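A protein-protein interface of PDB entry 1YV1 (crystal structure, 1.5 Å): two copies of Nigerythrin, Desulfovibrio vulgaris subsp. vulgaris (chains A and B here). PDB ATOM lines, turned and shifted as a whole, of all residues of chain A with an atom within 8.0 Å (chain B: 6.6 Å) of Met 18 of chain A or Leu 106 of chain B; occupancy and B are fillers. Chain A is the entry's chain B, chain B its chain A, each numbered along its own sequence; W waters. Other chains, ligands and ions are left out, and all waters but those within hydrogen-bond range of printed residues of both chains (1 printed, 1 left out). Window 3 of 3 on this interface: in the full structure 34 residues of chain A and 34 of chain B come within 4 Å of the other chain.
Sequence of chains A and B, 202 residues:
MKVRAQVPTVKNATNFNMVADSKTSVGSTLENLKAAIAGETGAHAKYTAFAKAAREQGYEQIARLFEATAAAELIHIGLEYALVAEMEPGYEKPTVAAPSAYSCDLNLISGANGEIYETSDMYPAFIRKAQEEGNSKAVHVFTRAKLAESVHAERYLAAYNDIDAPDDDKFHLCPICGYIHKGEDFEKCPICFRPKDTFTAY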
ATOM      1  N   THR A  14     -37.972 -13.390 -25.615  1.00  0.00           N
ATOM      2  CA  THR A  14     -37.424 -12.442 -24.657  1.00  0.00           C
ATOM      3  C   THR A  14     -35.916 -12.212 -24.725  1.00  0.00           C
ATOM      4  O   THR A  14     -35.317 -11.711 -23.772  1.00  0.00           O
ATOM      5  CB  THR A  14     -37.836 -12.821 -23.216  1.00  0.00           C
ATOM      6  OG1 THR A  14     -37.323 -14.116 -22.879  1.00  0.00           O
ATOM      7  CG2 THR A  14     -39.359 -12.846 -23.106  1.00  0.00           C
ATOM      8  N   ASN A  15     -35.300 -12.575 -25.848  1.00  0.00           N
ATOM      9  CA  ASN A  15     -33.869 -12.329 -26.014  1.00  0.00           C
ATOM     10  C   ASN A  15     -33.623 -11.396 -27.197  1.00  0.00           C
ATOM     11  O   ASN A  15     -32.656 -11.549 -27.940  1.00  0.00           O
ATOM     12  CB  ASN A  15     -33.065 -13.639 -26.167  1.00  0.00           C
ATOM     13  CG  ASN A  15     -33.515 -14.505 -27.339  1.00  0.00           C
ATOM     14  OD1 ASN A  15     -32.881 -15.525 -27.637  1.00  0.00           O
ATOM     15  ND2 ASN A  15     -34.599 -14.123 -27.995  1.00  0.00           N
ATOM     16  N   PHE A  16     -34.504 -10.409 -27.354  1.00  0.00           N
ATOM     17  CA  PHE A  16     -34.384  -9.445 -28.443  1.00  0.00           C
ATOM     18  C   PHE A  16     -33.934  -8.065 -27.981  1.00  0.00           C
ATOM     19  O   PHE A  16     -33.967  -7.104 -28.749  1.00  0.00           O
ATOM     20  CB  PHE A  16     -35.712  -9.322 -29.199  1.00  0.00           C
ATOM     21  CG  PHE A  16     -35.935 -10.413 -30.207  1.00  0.00           C
ATOM     22  CD1 PHE A  16     -36.094 -11.735 -29.802  1.00  0.00           C
ATOM     23  CD2 PHE A  16     -35.948 -10.124 -31.569  1.00  0.00           C
ATOM     24  CE1 PHE A  16     -36.261 -12.755 -30.739  1.00  0.00           C
ATOM     25  CE2 PHE A  16     -36.115 -11.138 -32.514  1.00  0.00           C
ATOM     26  CZ  PHE A  16     -36.270 -12.454 -32.098  1.00  0.00           C
ATOM     27  N   ASN A  17     -33.502  -7.959 -26.732  1.00  0.00           N
ATOM     28  CA  ASN A  17     -33.058  -6.671 -26.227  1.00  0.00           C
ATOM     29  C   ASN A  17     -31.685  -6.276 -26.767  1.00  0.00           C
ATOM     30  O   ASN A  17     -30.856  -7.129 -27.090  1.00  0.00           O
ATOM     31  CB  ASN A  17     -33.044  -6.683 -24.700  1.00  0.00           C
ATOM     32  CG  ASN A  17     -34.440  -6.798 -24.112  1.00  0.00           C
ATOM     33  OD1 ASN A  17     -35.313  -5.973 -24.394  1.00  0.00           O
ATOM     34  ND2 ASN A  17     -34.660  -7.822 -23.293  1.00  0.00           N
ATOM     35  N   MET A  18     -31.469  -4.971 -26.877  1.00  0.00           N
ATOM     36  CA  MET A  18     -30.211  -4.417 -27.369  1.00  0.00           C
ATOM     37  C   MET A  18     -29.387  -3.967 -26.166  1.00  0.00           C
ATOM     38  O   MET A  18     -29.922  -3.333 -25.257  1.00  0.00           O
ATOM     39  CB  MET A  18     -30.495  -3.203 -28.266  1.00  0.00           C
ATOM     40  CG  MET A  18     -29.245  -2.474 -28.741  1.00  0.00           C
ATOM     41  SD  MET A  18     -29.534  -0.788 -29.341  1.00  0.00           S
ATOM     42  CE  MET A  18     -29.616   0.100 -27.791  1.00  0.00           C
ATOM     43  N   VAL A  19     -28.098  -4.296 -26.151  1.00  0.00           N
ATOM     44  CA  VAL A  19     -27.247  -3.884 -25.042  1.00  0.00           C
ATOM     45  C   VAL A  19     -27.332  -2.363 -24.927  1.00  0.00           C
ATOM     46  O   VAL A  19     -27.273  -1.652 -25.932  1.00  0.00           O
ATOM     47  CB  VAL A  19     -25.772  -4.313 -25.259  1.00  0.00           C
ATOM     48  CG1 VAL A  19     -25.680  -5.828 -25.333  1.00  0.00           C
ATOM     49  CG2 VAL A  19     -25.217  -3.686 -26.522  1.00  0.00           C
ATOM     50  N   ALA A  20     -27.490  -1.867 -23.705  1.00  0.00           N
ATOM     51  CA  ALA A  20     -27.607  -0.429 -23.471  1.00  0.00           C
ATOM     52  C   ALA A  20     -26.486   0.400 -24.091  1.00  0.00           C
ATOM     53  O   ALA A  20     -26.744   1.431 -24.712  1.00  0.00           O
ATOM     54  CB  ALA A  20     -27.705  -0.149 -21.972  1.00  0.00           C
ATOM     55  N   ASP A  21     -25.245  -0.044 -23.926  1.00  0.00           N
ATOM     56  CA  ASP A  21     -24.115   0.683 -24.489  1.00  0.00           C
ATOM     57  C   ASP A  21     -23.811   0.130 -25.876  1.00  0.00           C
ATOM     58  O   ASP A  21     -22.810  -0.561 -26.084  1.00  0.00           O
ATOM     59  CB  ASP A  21     -22.888   0.542 -23.591  1.00  0.00           C
ATOM     60  CG  ASP A  21     -21.829   1.580 -23.896  1.00  0.00           C
ATOM     61  OD1 ASP A  21     -21.389   1.661 -25.065  1.00  0.00           O
ATOM     62  OD2 ASP A  21     -21.441   2.322 -22.966  1.00  0.00           O
ATOM     63  N   SER A  22     -24.687   0.446 -26.822  1.00  0.00           N
ATOM     64  CA  SER A  22     -24.569  -0.021 -28.199  1.00  0.00           C
ATOM     65  C   SER A  22     -23.434   0.577 -29.030  1.00  0.00           C
ATOM     66  O   SER A  22     -23.145   1.770 -28.952  1.00  0.00           O
ATOM     67  CB  SER A  22     -25.889   0.221 -28.929  1.00  0.00           C
ATOM     68  OG  SER A  22     -25.785  -0.157 -30.288  1.00  0.00           O
ATOM     69  N   LYS A  23     -22.808  -0.270 -29.844  1.00  0.00           N
ATOM     70  CA  LYS A  23     -21.716   0.147 -30.718  1.00  0.00           C
ATOM     71  C   LYS A  23     -22.257   0.229 -32.143  1.00  0.00           C
ATOM     72  O   LYS A  23     -21.501   0.139 -33.112  1.00  0.00           O
ATOM     73  CB  LYS A  23     -20.585  -0.884 -30.684  1.00  0.00           C
ATOM     74  CG  LYS A  23     -19.953  -1.106 -29.319  1.00  0.00           C
ATOM     75  CD  LYS A  23     -18.882  -2.183 -29.400  1.00  0.00           C
ATOM     76  CE  LYS A  23     -18.176  -2.373 -28.070  1.00  0.00           C
ATOM     77  NZ  LYS A  23     -17.135  -3.434 -28.162  1.00  0.00           N
ATOM     78  N   THR A  24     -23.565   0.418 -32.269  1.00  0.00           N
ATOM     79  CA  THR A  24     -24.181   0.452 -33.587  1.00  0.00           C
ATOM     80  C   THR A  24     -24.810   1.776 -34.009  1.00  0.00           C
ATOM     81  O   THR A  24     -25.656   2.331 -33.305  1.00  0.00           O
ATOM     82  CB  THR A  24     -25.254  -0.656 -33.693  1.00  0.00           C
ATOM     83  OG1 THR A  24     -24.681  -1.915 -33.315  1.00  0.00           O
ATOM     84  CG2 THR A  24     -25.784  -0.760 -35.114  1.00  0.00           C
ATOM     85  N   VAL A  26     -27.348   3.737 -35.966  1.00  0.00           N
ATOM     86  CA  VAL A  26     -28.662   3.418 -36.511  1.00  0.00           C
ATOM     87  C   VAL A  26     -29.228   4.541 -37.365  1.00  0.00           C
ATOM     88  O   VAL A  26     -29.338   5.685 -36.916  1.00  0.00           O
ATOM     89  CB  VAL A  26     -29.667   3.113 -35.384  1.00  0.00           C
ATOM     90  CG1 VAL A  26     -31.037   2.807 -35.978  1.00  0.00           C
ATOM     91  CG2 VAL A  26     -29.175   1.944 -34.554  1.00  0.00           C
ATOM     92  N   TYR A 117     -22.033  -9.846 -31.027  1.00  0.00           N
ATOM     93  CA  TYR A 117     -22.286  -8.437 -31.295  1.00  0.00           C
ATOM     94  C   TYR A 117     -23.535  -8.294 -32.161  1.00  0.00           C
ATOM     95  O   TYR A 117     -24.399  -7.457 -31.902  1.00  0.00           O
ATOM     96  CB  TYR A 117     -21.082  -7.802 -32.007  1.00  0.00           C
ATOM     97  CG  TYR A 117     -21.431  -6.516 -32.723  1.00  0.00           C
ATOM     98  CD1 TYR A 117     -21.569  -6.484 -34.111  1.00  0.00           C
ATOM     99  CD2 TYR A 117     -21.704  -5.351 -32.005  1.00  0.00           C
ATOM    100  CE1 TYR A 117     -21.979  -5.323 -34.768  1.00  0.00           C
ATOM    101  CE2 TYR A 117     -22.115  -4.189 -32.651  1.00  0.00           C
ATOM    102  CZ  TYR A 117     -22.254  -4.183 -34.032  1.00  0.00           C
ATOM    103  OH  TYR A 117     -22.701  -3.045 -34.670  1.00  0.00           O
ATOM    104  N   THR A 119     -26.111 -10.470 -32.645  1.00  0.00           N
ATOM    105  CA  THR A 119     -27.343 -10.931 -32.027  1.00  0.00           C
ATOM    106  C   THR A 119     -27.819 -10.117 -30.830  1.00  0.00           C
ATOM    107  O   THR A 119     -29.019 -10.063 -30.565  1.00  0.00           O
ATOM    108  CB  THR A 119     -27.226 -12.421 -31.610  1.00  0.00           C
ATOM    109  OG1 THR A 119     -28.534 -13.003 -31.553  1.00  0.00           O
ATOM    110  CG2 THR A 119     -26.559 -12.559 -30.240  1.00  0.00           C
ATOM    111  N   SER A 120     -26.896  -9.464 -30.130  1.00  0.00           N
ATOM    112  CA  SER A 120     -27.253  -8.700 -28.934  1.00  0.00           C
ATOM    113  C   SER A 120     -27.119  -7.189 -29.068  1.00  0.00           C
ATOM    114  O   SER A 120     -27.500  -6.450 -28.157  1.00  0.00           O
ATOM    115  CB  SER A 120     -26.378  -9.147 -27.761  1.00  0.00           C
ATOM    116  OG  SER A 120     -25.043  -8.703 -27.945  1.00  0.00           O
ATOM    117  N   ASP A 121     -26.577  -6.730 -30.187  1.00  0.00           N
ATOM    118  CA  ASP A 121     -26.370  -5.304 -30.383  1.00  0.00           C
ATOM    119  C   ASP A 121     -26.926  -4.815 -31.716  1.00  0.00           C
ATOM    120  O   ASP A 121     -27.992  -4.197 -31.765  1.00  0.00           O
ATOM    121  CB  ASP A 121     -24.867  -4.999 -30.293  1.00  0.00           C
ATOM    122  CG  ASP A 121     -24.558  -3.511 -30.280  1.00  0.00           C
ATOM    123  OD1 ASP A 121     -25.314  -2.726 -30.889  1.00  0.00           O
ATOM    124  OD2 ASP A 121     -23.537  -3.130 -29.667  1.00  0.00           O
ATOM    125  N   MET A 122     -26.219  -5.118 -32.800  1.00  0.00           N
ATOM    126  CA  MET A 122     -26.630  -4.656 -34.120  1.00  0.00           C
ATOM    127  C   MET A 122     -28.037  -5.035 -34.565  1.00  0.00           C
ATOM    128  O   MET A 122     -28.853  -4.156 -34.843  1.00  0.00           O
ATOM    129  CB  MET A 122     -25.632  -5.115 -35.184  1.00  0.00           C
ATOM    130  CG  MET A 122     -25.879  -4.452 -36.532  1.00  0.00           C
ATOM    131  SD  MET A 122     -24.963  -5.197 -37.878  1.00  0.00           S
ATOM    132  CE  MET A 122     -25.993  -6.622 -38.253  1.00  0.00           C
ATOM    133  N   TYR A 123     -28.338  -6.328 -34.651  1.00  0.00           N
ATOM    134  CA  TYR A 123     -29.670  -6.706 -35.096  1.00  0.00           C
ATOM    135  C   TYR A 123     -30.784  -6.241 -34.162  1.00  0.00           C
ATOM    136  O   TYR A 123     -31.828  -5.795 -34.632  1.00  0.00           O
ATOM    137  CB  TYR A 123     -29.732  -8.212 -35.400  1.00  0.00           C
ATOM    138  CG  TYR A 123     -29.183  -8.515 -36.788  1.00  0.00           C
ATOM    139  CD1 TYR A 123     -28.182  -9.469 -36.979  1.00  0.00           C
ATOM    140  CD2 TYR A 123     -29.648  -7.816 -37.905  1.00  0.00           C
ATOM    141  CE1 TYR A 123     -27.651  -9.716 -38.257  1.00  0.00           C
ATOM    142  CE2 TYR A 123     -29.129  -8.053 -39.179  1.00  0.00           C
ATOM    143  CZ  TYR A 123     -28.131  -9.003 -39.348  1.00  0.00           C
ATOM    144  OH  TYR A 123     -27.616  -9.222 -40.605  1.00  0.00           O
ATOM    145  N   PRO A 124     -30.589  -6.330 -32.835  1.00  0.00           N
ATOM    146  CA  PRO A 124     -31.679  -5.850 -31.978  1.00  0.00           C
ATOM    147  C   PRO A 124     -31.935  -4.360 -32.227  1.00  0.00           C
ATOM    148  O   PRO A 124     -33.080  -3.909 -32.210  1.00  0.00           O
ATOM    149  CB  PRO A 124     -31.152  -6.123 -30.575  1.00  0.00           C
ATOM    150  CG  PRO A 124     -30.426  -7.409 -30.765  1.00  0.00           C
ATOM    151  CD  PRO A 124     -29.655  -7.168 -32.060  1.00  0.00           C
ATOM    152  N   ALA A 125     -30.865  -3.602 -32.469  1.00  0.00           N
ATOM    153  CA  ALA A 125     -30.985  -2.169 -32.737  1.00  0.00           C
ATOM    154  C   ALA A 125     -31.743  -1.939 -34.042  1.00  0.00           C
ATOM    155  O   ALA A 125     -32.628  -1.083 -34.117  1.00  0.00           O
ATOM    156  CB  ALA A 125     -29.605  -1.534 -32.821  1.00  0.00           C
ATOM    157  N   PHE A 126     -31.395  -2.709 -35.069  1.00  0.00           N
ATOM    158  CA  PHE A 126     -32.043  -2.580 -36.368  1.00  0.00           C
ATOM    159  C   PHE A 126     -33.497  -3.040 -36.330  1.00  0.00           C
ATOM    160  O   PHE A 126     -34.354  -2.457 -36.995  1.00  0.00           O
ATOM    161  CB  PHE A 126     -31.281  -3.384 -37.423  1.00  0.00           C
ATOM    162  CG  PHE A 126     -29.953  -2.788 -37.809  1.00  0.00           C
ATOM    163  CD1 PHE A 126     -29.122  -3.451 -38.707  1.00  0.00           C
ATOM    164  CD2 PHE A 126     -29.534  -1.564 -37.290  1.00  0.00           C
ATOM    165  CE1 PHE A 126     -27.898  -2.909 -39.083  1.00  0.00           C
ATOM    166  CE2 PHE A 126     -28.305  -1.013 -37.664  1.00  0.00           C
ATOM    167  CZ  PHE A 126     -27.490  -1.686 -38.559  1.00  0.00           C
ATOM    168  N   ARG A 128     -35.514  -2.978 -33.698  1.00  0.00           N
ATOM    169  CA  ARG A 128     -36.274  -1.970 -32.978  1.00  0.00           C
ATOM    170  C   ARG A 128     -36.593  -0.776 -33.875  1.00  0.00           C
ATOM    171  O   ARG A 128     -37.720  -0.276 -33.868  1.00  0.00           O
ATOM    172  CB  ARG A 128     -35.496  -1.505 -31.746  1.00  0.00           C
ATOM    173  CG  ARG A 128     -36.215  -0.440 -30.944  1.00  0.00           C
ATOM    174  CD  ARG A 128     -37.514  -0.945 -30.334  1.00  0.00           C
ATOM    175  NE  ARG A 128     -38.382   0.172 -29.964  1.00  0.00           N
ATOM    176  CZ  ARG A 128     -39.452   0.073 -29.182  1.00  0.00           C
ATOM    177  NH1 ARG A 128     -39.802  -1.102 -28.670  1.00  0.00           N
ATOM    178  NH2 ARG A 128     -40.177   1.153 -28.915  1.00  0.00           N
ATOM    179  N   LYS A 146     -30.843 -12.402 -36.819  1.00  0.00           N
ATOM    180  CA  LYS A 146     -30.528 -12.280 -35.397  1.00  0.00           C
ATOM    181  C   LYS A 146     -30.568 -13.612 -34.658  1.00  0.00           C
ATOM    182  O   LYS A 146     -29.651 -13.942 -33.898  1.00  0.00           O
ATOM    183  CB  LYS A 146     -31.494 -11.278 -34.743  1.00  0.00           C
ATOM    184  CG  LYS A 146     -31.354 -11.098 -33.226  1.00  0.00           C
ATOM    185  CD  LYS A 146     -32.246 -12.065 -32.445  1.00  0.00           C
ATOM    186  CE  LYS A 146     -32.312 -11.712 -30.959  1.00  0.00           C
ATOM    187  NZ  LYS A 146     -31.036 -11.981 -30.230  1.00  0.00           N
ATOM    188  N   PHE B  50     -27.025 -11.154 -11.088  1.00  0.00           N
ATOM    189  CA  PHE B  50     -27.790 -11.626 -12.238  1.00  0.00           C
ATOM    190  C   PHE B  50     -28.789 -12.708 -11.834  1.00  0.00           C
ATOM    191  O   PHE B  50     -29.879 -12.803 -12.405  1.00  0.00           O
ATOM    192  CB  PHE B  50     -26.851 -12.165 -13.324  1.00  0.00           C
ATOM    193  CG  PHE B  50     -26.062 -11.098 -14.043  1.00  0.00           C
ATOM    194  CD1 PHE B  50     -25.175 -11.449 -15.056  1.00  0.00           C
ATOM    195  CD2 PHE B  50     -26.210  -9.748 -13.726  1.00  0.00           C
ATOM    196  CE1 PHE B  50     -24.450 -10.477 -15.743  1.00  0.00           C
ATOM    197  CE2 PHE B  50     -25.488  -8.769 -14.411  1.00  0.00           C
ATOM    198  CZ  PHE B  50     -24.607  -9.138 -15.421  1.00  0.00           C
ATOM    199  N   TYR B 102     -29.307  -5.953 -15.739  1.00  0.00           N
ATOM    200  CA  TYR B 102     -30.245  -5.548 -16.777  1.00  0.00           C
ATOM    201  C   TYR B 102     -31.192  -6.704 -17.062  1.00  0.00           C
ATOM    202  O   TYR B 102     -31.363  -7.576 -16.217  1.00  0.00           O
ATOM    203  CB  TYR B 102     -29.474  -5.143 -18.034  1.00  0.00           C
ATOM    204  CG  TYR B 102     -28.540  -3.978 -17.788  1.00  0.00           C
ATOM    205  CD1 TYR B 102     -27.246  -4.180 -17.299  1.00  0.00           C
ATOM    206  CD2 TYR B 102     -28.969  -2.667 -17.997  1.00  0.00           C
ATOM    207  CE1 TYR B 102     -26.403  -3.097 -17.023  1.00  0.00           C
ATOM    208  CE2 TYR B 102     -28.139  -1.583 -17.720  1.00  0.00           C
ATOM    209  CZ  TYR B 102     -26.860  -1.802 -17.235  1.00  0.00           C
ATOM    210  OH  TYR B 102     -26.049  -0.726 -16.955  1.00  0.00           O
ATOM    211  N   SER B 103     -31.820  -6.724 -18.234  1.00  0.00           N
ATOM    212  CA  SER B 103     -32.729  -7.825 -18.534  1.00  0.00           C
ATOM    213  C   SER B 103     -31.944  -9.132 -18.573  1.00  0.00           C
ATOM    214  O   SER B 103     -30.744  -9.137 -18.848  1.00  0.00           O
ATOM    215  CB  SER B 103     -33.467  -7.591 -19.858  1.00  0.00           C
ATOM    216  OG  SER B 103     -32.578  -7.360 -20.933  1.00  0.00           O
ATOM    217  N   CYS B 104     -32.624 -10.237 -18.291  1.00  0.00           N
ATOM    218  CA  CYS B 104     -31.978 -11.544 -18.252  1.00  0.00           C
ATOM    219  C   CYS B 104     -31.158 -11.884 -19.492  1.00  0.00           C
ATOM    220  O   CYS B 104     -30.015 -12.337 -19.378  1.00  0.00           O
ATOM    221  CB  CYS B 104     -33.023 -12.636 -18.017  1.00  0.00           C
ATOM    222  SG  CYS B 104     -32.312 -14.258 -17.657  1.00  0.00           S
ATOM    223  N   ASP B 105     -31.727 -11.670 -20.673  1.00  0.00           N
ATOM    224  CA  ASP B 105     -31.001 -11.988 -21.896  1.00  0.00           C
ATOM    225  C   ASP B 105     -29.686 -11.217 -21.990  1.00  0.00           C
ATOM    226  O   ASP B 105     -28.644 -11.788 -22.318  1.00  0.00           O
ATOM    227  CB  ASP B 105     -31.883 -11.749 -23.140  1.00  0.00           C
ATOM    228  CG  ASP B 105     -32.312 -10.299 -23.313  1.00  0.00           C
ATOM    229  OD1 ASP B 105     -32.685  -9.656 -22.312  1.00  0.00           O
ATOM    230  OD2 ASP B 105     -32.300  -9.814 -24.469  1.00  0.00           O
ATOM    231  N   LEU B 106     -29.725  -9.927 -21.683  1.00  0.00           N
ATOM    232  CA  LEU B 106     -28.523  -9.105 -21.731  1.00  0.00           C
ATOM    233  C   LEU B 106     -27.499  -9.536 -20.685  1.00  0.00           C
ATOM    234  O   LEU B 106     -26.291  -9.461 -20.924  1.00  0.00           O
ATOM    235  CB  LEU B 106     -28.886  -7.631 -21.542  1.00  0.00           C
ATOM    236  CG  LEU B 106     -29.750  -7.052 -22.665  1.00  0.00           C
ATOM    237  CD1 LEU B 106     -30.082  -5.603 -22.343  1.00  0.00           C
ATOM    238  CD2 LEU B 106     -29.017  -7.154 -24.001  1.00  0.00           C
ATOM    239  N   ASN B 107     -27.978  -9.979 -19.525  1.00  0.00           N
ATOM    240  CA  ASN B 107     -27.075 -10.431 -18.474  1.00  0.00           C
ATOM    241  C   ASN B 107     -26.340 -11.696 -18.925  1.00  0.00           C
ATOM    242  O   ASN B 107     -25.162 -11.875 -18.624  1.00  0.00           O
ATOM    243  CB  ASN B 107     -27.840 -10.700 -17.172  1.00  0.00           C
ATOM    244  CG  ASN B 107     -28.413  -9.433 -16.556  1.00  0.00           C
ATOM    245  OD1 ASN B 107     -27.933  -8.327 -16.816  1.00  0.00           O
ATOM    246  ND2 ASN B 107     -29.430  -9.594 -15.719  1.00  0.00           N
ATOM    247  N   LEU B 108     -27.038 -12.572 -19.648  1.00  0.00           N
ATOM    248  CA  LEU B 108     -26.417 -13.795 -20.152  1.00  0.00           C
ATOM    249  C   LEU B 108     -25.305 -13.433 -21.133  1.00  0.00           C
ATOM    250  O   LEU B 108     -24.235 -14.048 -21.133  1.00  0.00           O
ATOM    251  CB  LEU B 108     -27.461 -14.673 -20.847  1.00  0.00           C
ATOM    252  CG  LEU B 108     -28.385 -15.464 -19.918  1.00  0.00           C
ATOM    253  CD1 LEU B 108     -29.564 -16.040 -20.696  1.00  0.00           C
ATOM    254  CD2 LEU B 108     -27.587 -16.576 -19.242  1.00  0.00           C
ATOM    255  N   ILE B 109     -25.558 -12.429 -21.967  1.00  0.00           N
ATOM    256  CA  ILE B 109     -24.574 -11.975 -22.943  1.00  0.00           C
ATOM    257  C   ILE B 109     -23.385 -11.331 -22.235  1.00  0.00           C
ATOM    258  O   ILE B 109     -22.236 -11.592 -22.584  1.00  0.00           O
ATOM    259  CB  ILE B 109     -25.201 -10.963 -23.933  1.00  0.00           C
ATOM    260  CG1 ILE B 109     -26.238 -11.670 -24.813  1.00  0.00           C
ATOM    261  CG2 ILE B 109     -24.112 -10.311 -24.786  1.00  0.00           C
ATOM    262  CD1 ILE B 109     -25.654 -12.709 -25.778  1.00  0.00           C
ATOM    263  N   SER B 110     -23.665 -10.491 -21.240  1.00  0.00           N
ATOM    264  CA  SER B 110     -22.605  -9.837 -20.476  1.00  0.00           C
ATOM    265  C   SER B 110     -21.719 -10.910 -19.855  1.00  0.00           C
ATOM    266  O   SER B 110     -20.488 -10.795 -19.845  1.00  0.00           O
ATOM    267  CB  SER B 110     -23.201  -8.965 -19.366  1.00  0.00           C
ATOM    268  OG  SER B 110     -22.172  -8.356 -18.604  1.00  0.00           O
ATOM    269  N   GLY B 111     -22.357 -11.955 -19.331  1.00  0.00           N
ATOM    270  CA  GLY B 111     -21.619 -13.050 -18.729  1.00  0.00           C
ATOM    271  C   GLY B 111     -20.741 -13.738 -19.757  1.00  0.00           C
ATOM    272  O   GLY B 111     -19.552 -13.945 -19.525  1.00  0.00           O
ATOM    273  N   TYR B 160     -29.202 -18.517 -23.448  1.00  0.00           N
ATOM    274  CA  TYR B 160     -29.699 -17.362 -24.187  1.00  0.00           C
ATOM    275  C   TYR B 160     -30.552 -17.842 -25.365  1.00  0.00           C
ATOM    276  O   TYR B 160     -31.640 -17.323 -25.604  1.00  0.00           O
ATOM    277  CB  TYR B 160     -28.511 -16.541 -24.697  1.00  0.00           C
ATOM    278  CG  TYR B 160     -28.854 -15.306 -25.502  1.00  0.00           C
ATOM    279  CD1 TYR B 160     -29.069 -14.074 -24.880  1.00  0.00           C
ATOM    280  CD2 TYR B 160     -28.898 -15.355 -26.897  1.00  0.00           C
ATOM    281  CE1 TYR B 160     -29.304 -12.918 -25.630  1.00  0.00           C
ATOM    282  CE2 TYR B 160     -29.133 -14.212 -27.652  1.00  0.00           C
ATOM    283  CZ  TYR B 160     -29.332 -12.996 -27.013  1.00  0.00           C
ATOM    284  OH  TYR B 160     -29.535 -11.860 -27.764  1.00  0.00           O
ATOM    285  N   ILE B 163     -33.816 -19.167 -23.982  1.00  0.00           N
ATOM    286  CA  ILE B 163     -34.340 -18.357 -22.888  1.00  0.00           C
ATOM    287  C   ILE B 163     -35.835 -18.565 -22.633  1.00  0.00           C
ATOM    288  O   ILE B 163     -36.292 -18.481 -21.491  1.00  0.00           O
ATOM    289  CB  ILE B 163     -34.051 -16.853 -23.126  1.00  0.00           C
ATOM    290  CG1 ILE B 163     -34.318 -16.070 -21.841  1.00  0.00           C
ATOM    291  CG2 ILE B 163     -34.902 -16.317 -24.271  1.00  0.00           C
ATOM    292  CD1 ILE B 163     -33.773 -14.659 -21.860  1.00  0.00           C
HETATM  293  O   HOH W   1     -35.050 -11.343 -20.913  1.00  0.00           O
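Of the 23 printed residues of chain A, 9 touch a printed residue of chain B.
Printed residues of chain A that touch a printed residue of chain B: Thr 14, Asn 15, Phe 16, Asn 17, Met 18, Val 19, Thr 119, Ser 120 and Lys 146.
Hydrophobic or aromatic side chains of chain A that line the printed part of chain B: Val 19.
Printed residues of chain B that touch a printed residue of chain A: Ser 103, Asp 105, Leu 106, Ile 109, Tyr 160 and Ile 163.
Among the printed residues, 14 pairs touch across the chains.
Among the printed residues, pairs that only touch across the chains: Asn 15 of chain A with Asp 105 of chain B, Thr 14 of chain A with Asp 105 of chain B, Thr 14 of chain A with Ile 163 of chain B, Asn 17 of chain A with Leu 106 of chain B, Ser 120 of chain A with Ile 109 of chain B, Phe 16 of chain A with Asp 105 of chain B, Val 19 of chain A with Leu 106 of chain B, Met 18 of chain A with Leu 106 of chain B and Asn 15 of chain A with Ile 163 of chain B.
No position is printed for both chains.
Of the 14 pairs that touch across the chains among the printed residues, none has its exchanged pair printed and touching as well.
The side-chain hydroxyl (OG) of Ser 103 of chain B lies within hydrogen-bond range of the side-chain carboxylate (OD1) of Asp 105 of chain B (2.7 Å).
The backbone carbonyl oxygen (O) of Ser 103 of chain B lies close to the side-chain amide nitrogen (ND2) of Asn 107 of chain B (3.4 Å).
The side-chain amino group of Lys 146 of chain A sits at hydrogen-bond distance from the backbone carbonyl oxygen of Asn 15 of chain A, 2.8 Å away.
The backbone NH (N) of Val 19 of chain A sits at hydrogen-bond distance from the backbone carbonyl oxygen (O) of Ser 120 of chain A, at 3.0 Å.
The backbone carbonyl oxygen (O) of Lys 146 of chain A sits at hydrogen-bond distance from the side-chain hydroxyl (OG1) of Thr 119 of chain A (2.8 Å).
Printed residues of chain A within 4 Å of Ile 109 of chain B: Ser 120 (3.7 Å).
Printed residues of chain B within 4 Å of Lys 146 of chain A: Tyr 160 (2.9 Å).
Of the printed residues of chain B, Ser 120 of chain A touches Ile 109 (3.7 Å).
Printed residues of chain A within 4 Å of Ser 103 of chain B: Asn 17.
Of the printed residues of chain B, Thr 14 of chain A touches Asp 105 and Ile 163.
The nearest residue of chain B that does not touch Met 18 of chain A is Asp 105 of chain B (5.5 Å).
The nearest printed residue of chain A that does not touch Leu 106 of chain B is Ser 120 of chain A (4.5 Å).
The nearest printed residue of chain B that does not touch Asn 17 of chain A is Tyr 160 of chain B (5.0 Å).
Water W1 bridges the backbone carbonyl oxygen (O) of Thr 14 of chain A (2.9 Å) and the side-chain carboxylate (OD1) of Asp 105 of chain B (3.2 Å).
The side-chain hydroxyl of Ser 103 of chain B lies within hydrogen-bond range of the side-chain amide nitrogen of Asn 17 of chain A (3.2 Å).
The side-chain carboxylate (OD1) of Asp 105 of chain B lies within hydrogen-bond range of the side-chain amide nitrogen (ND2) of Asn 17 of chain A, 2.9 Å away.
O of Tyr 160 of chain B lies close to OD1 of Asn 15 of chain A, 3.0 Å away.
OH of Tyr 160 of chain B is in hydrogen-bond range of O of Thr 119 of chain A.
OH of Tyr 160 of chain B is in hydrogen-bond range of NZ of Lys 146 of chain A (2.9 Å).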
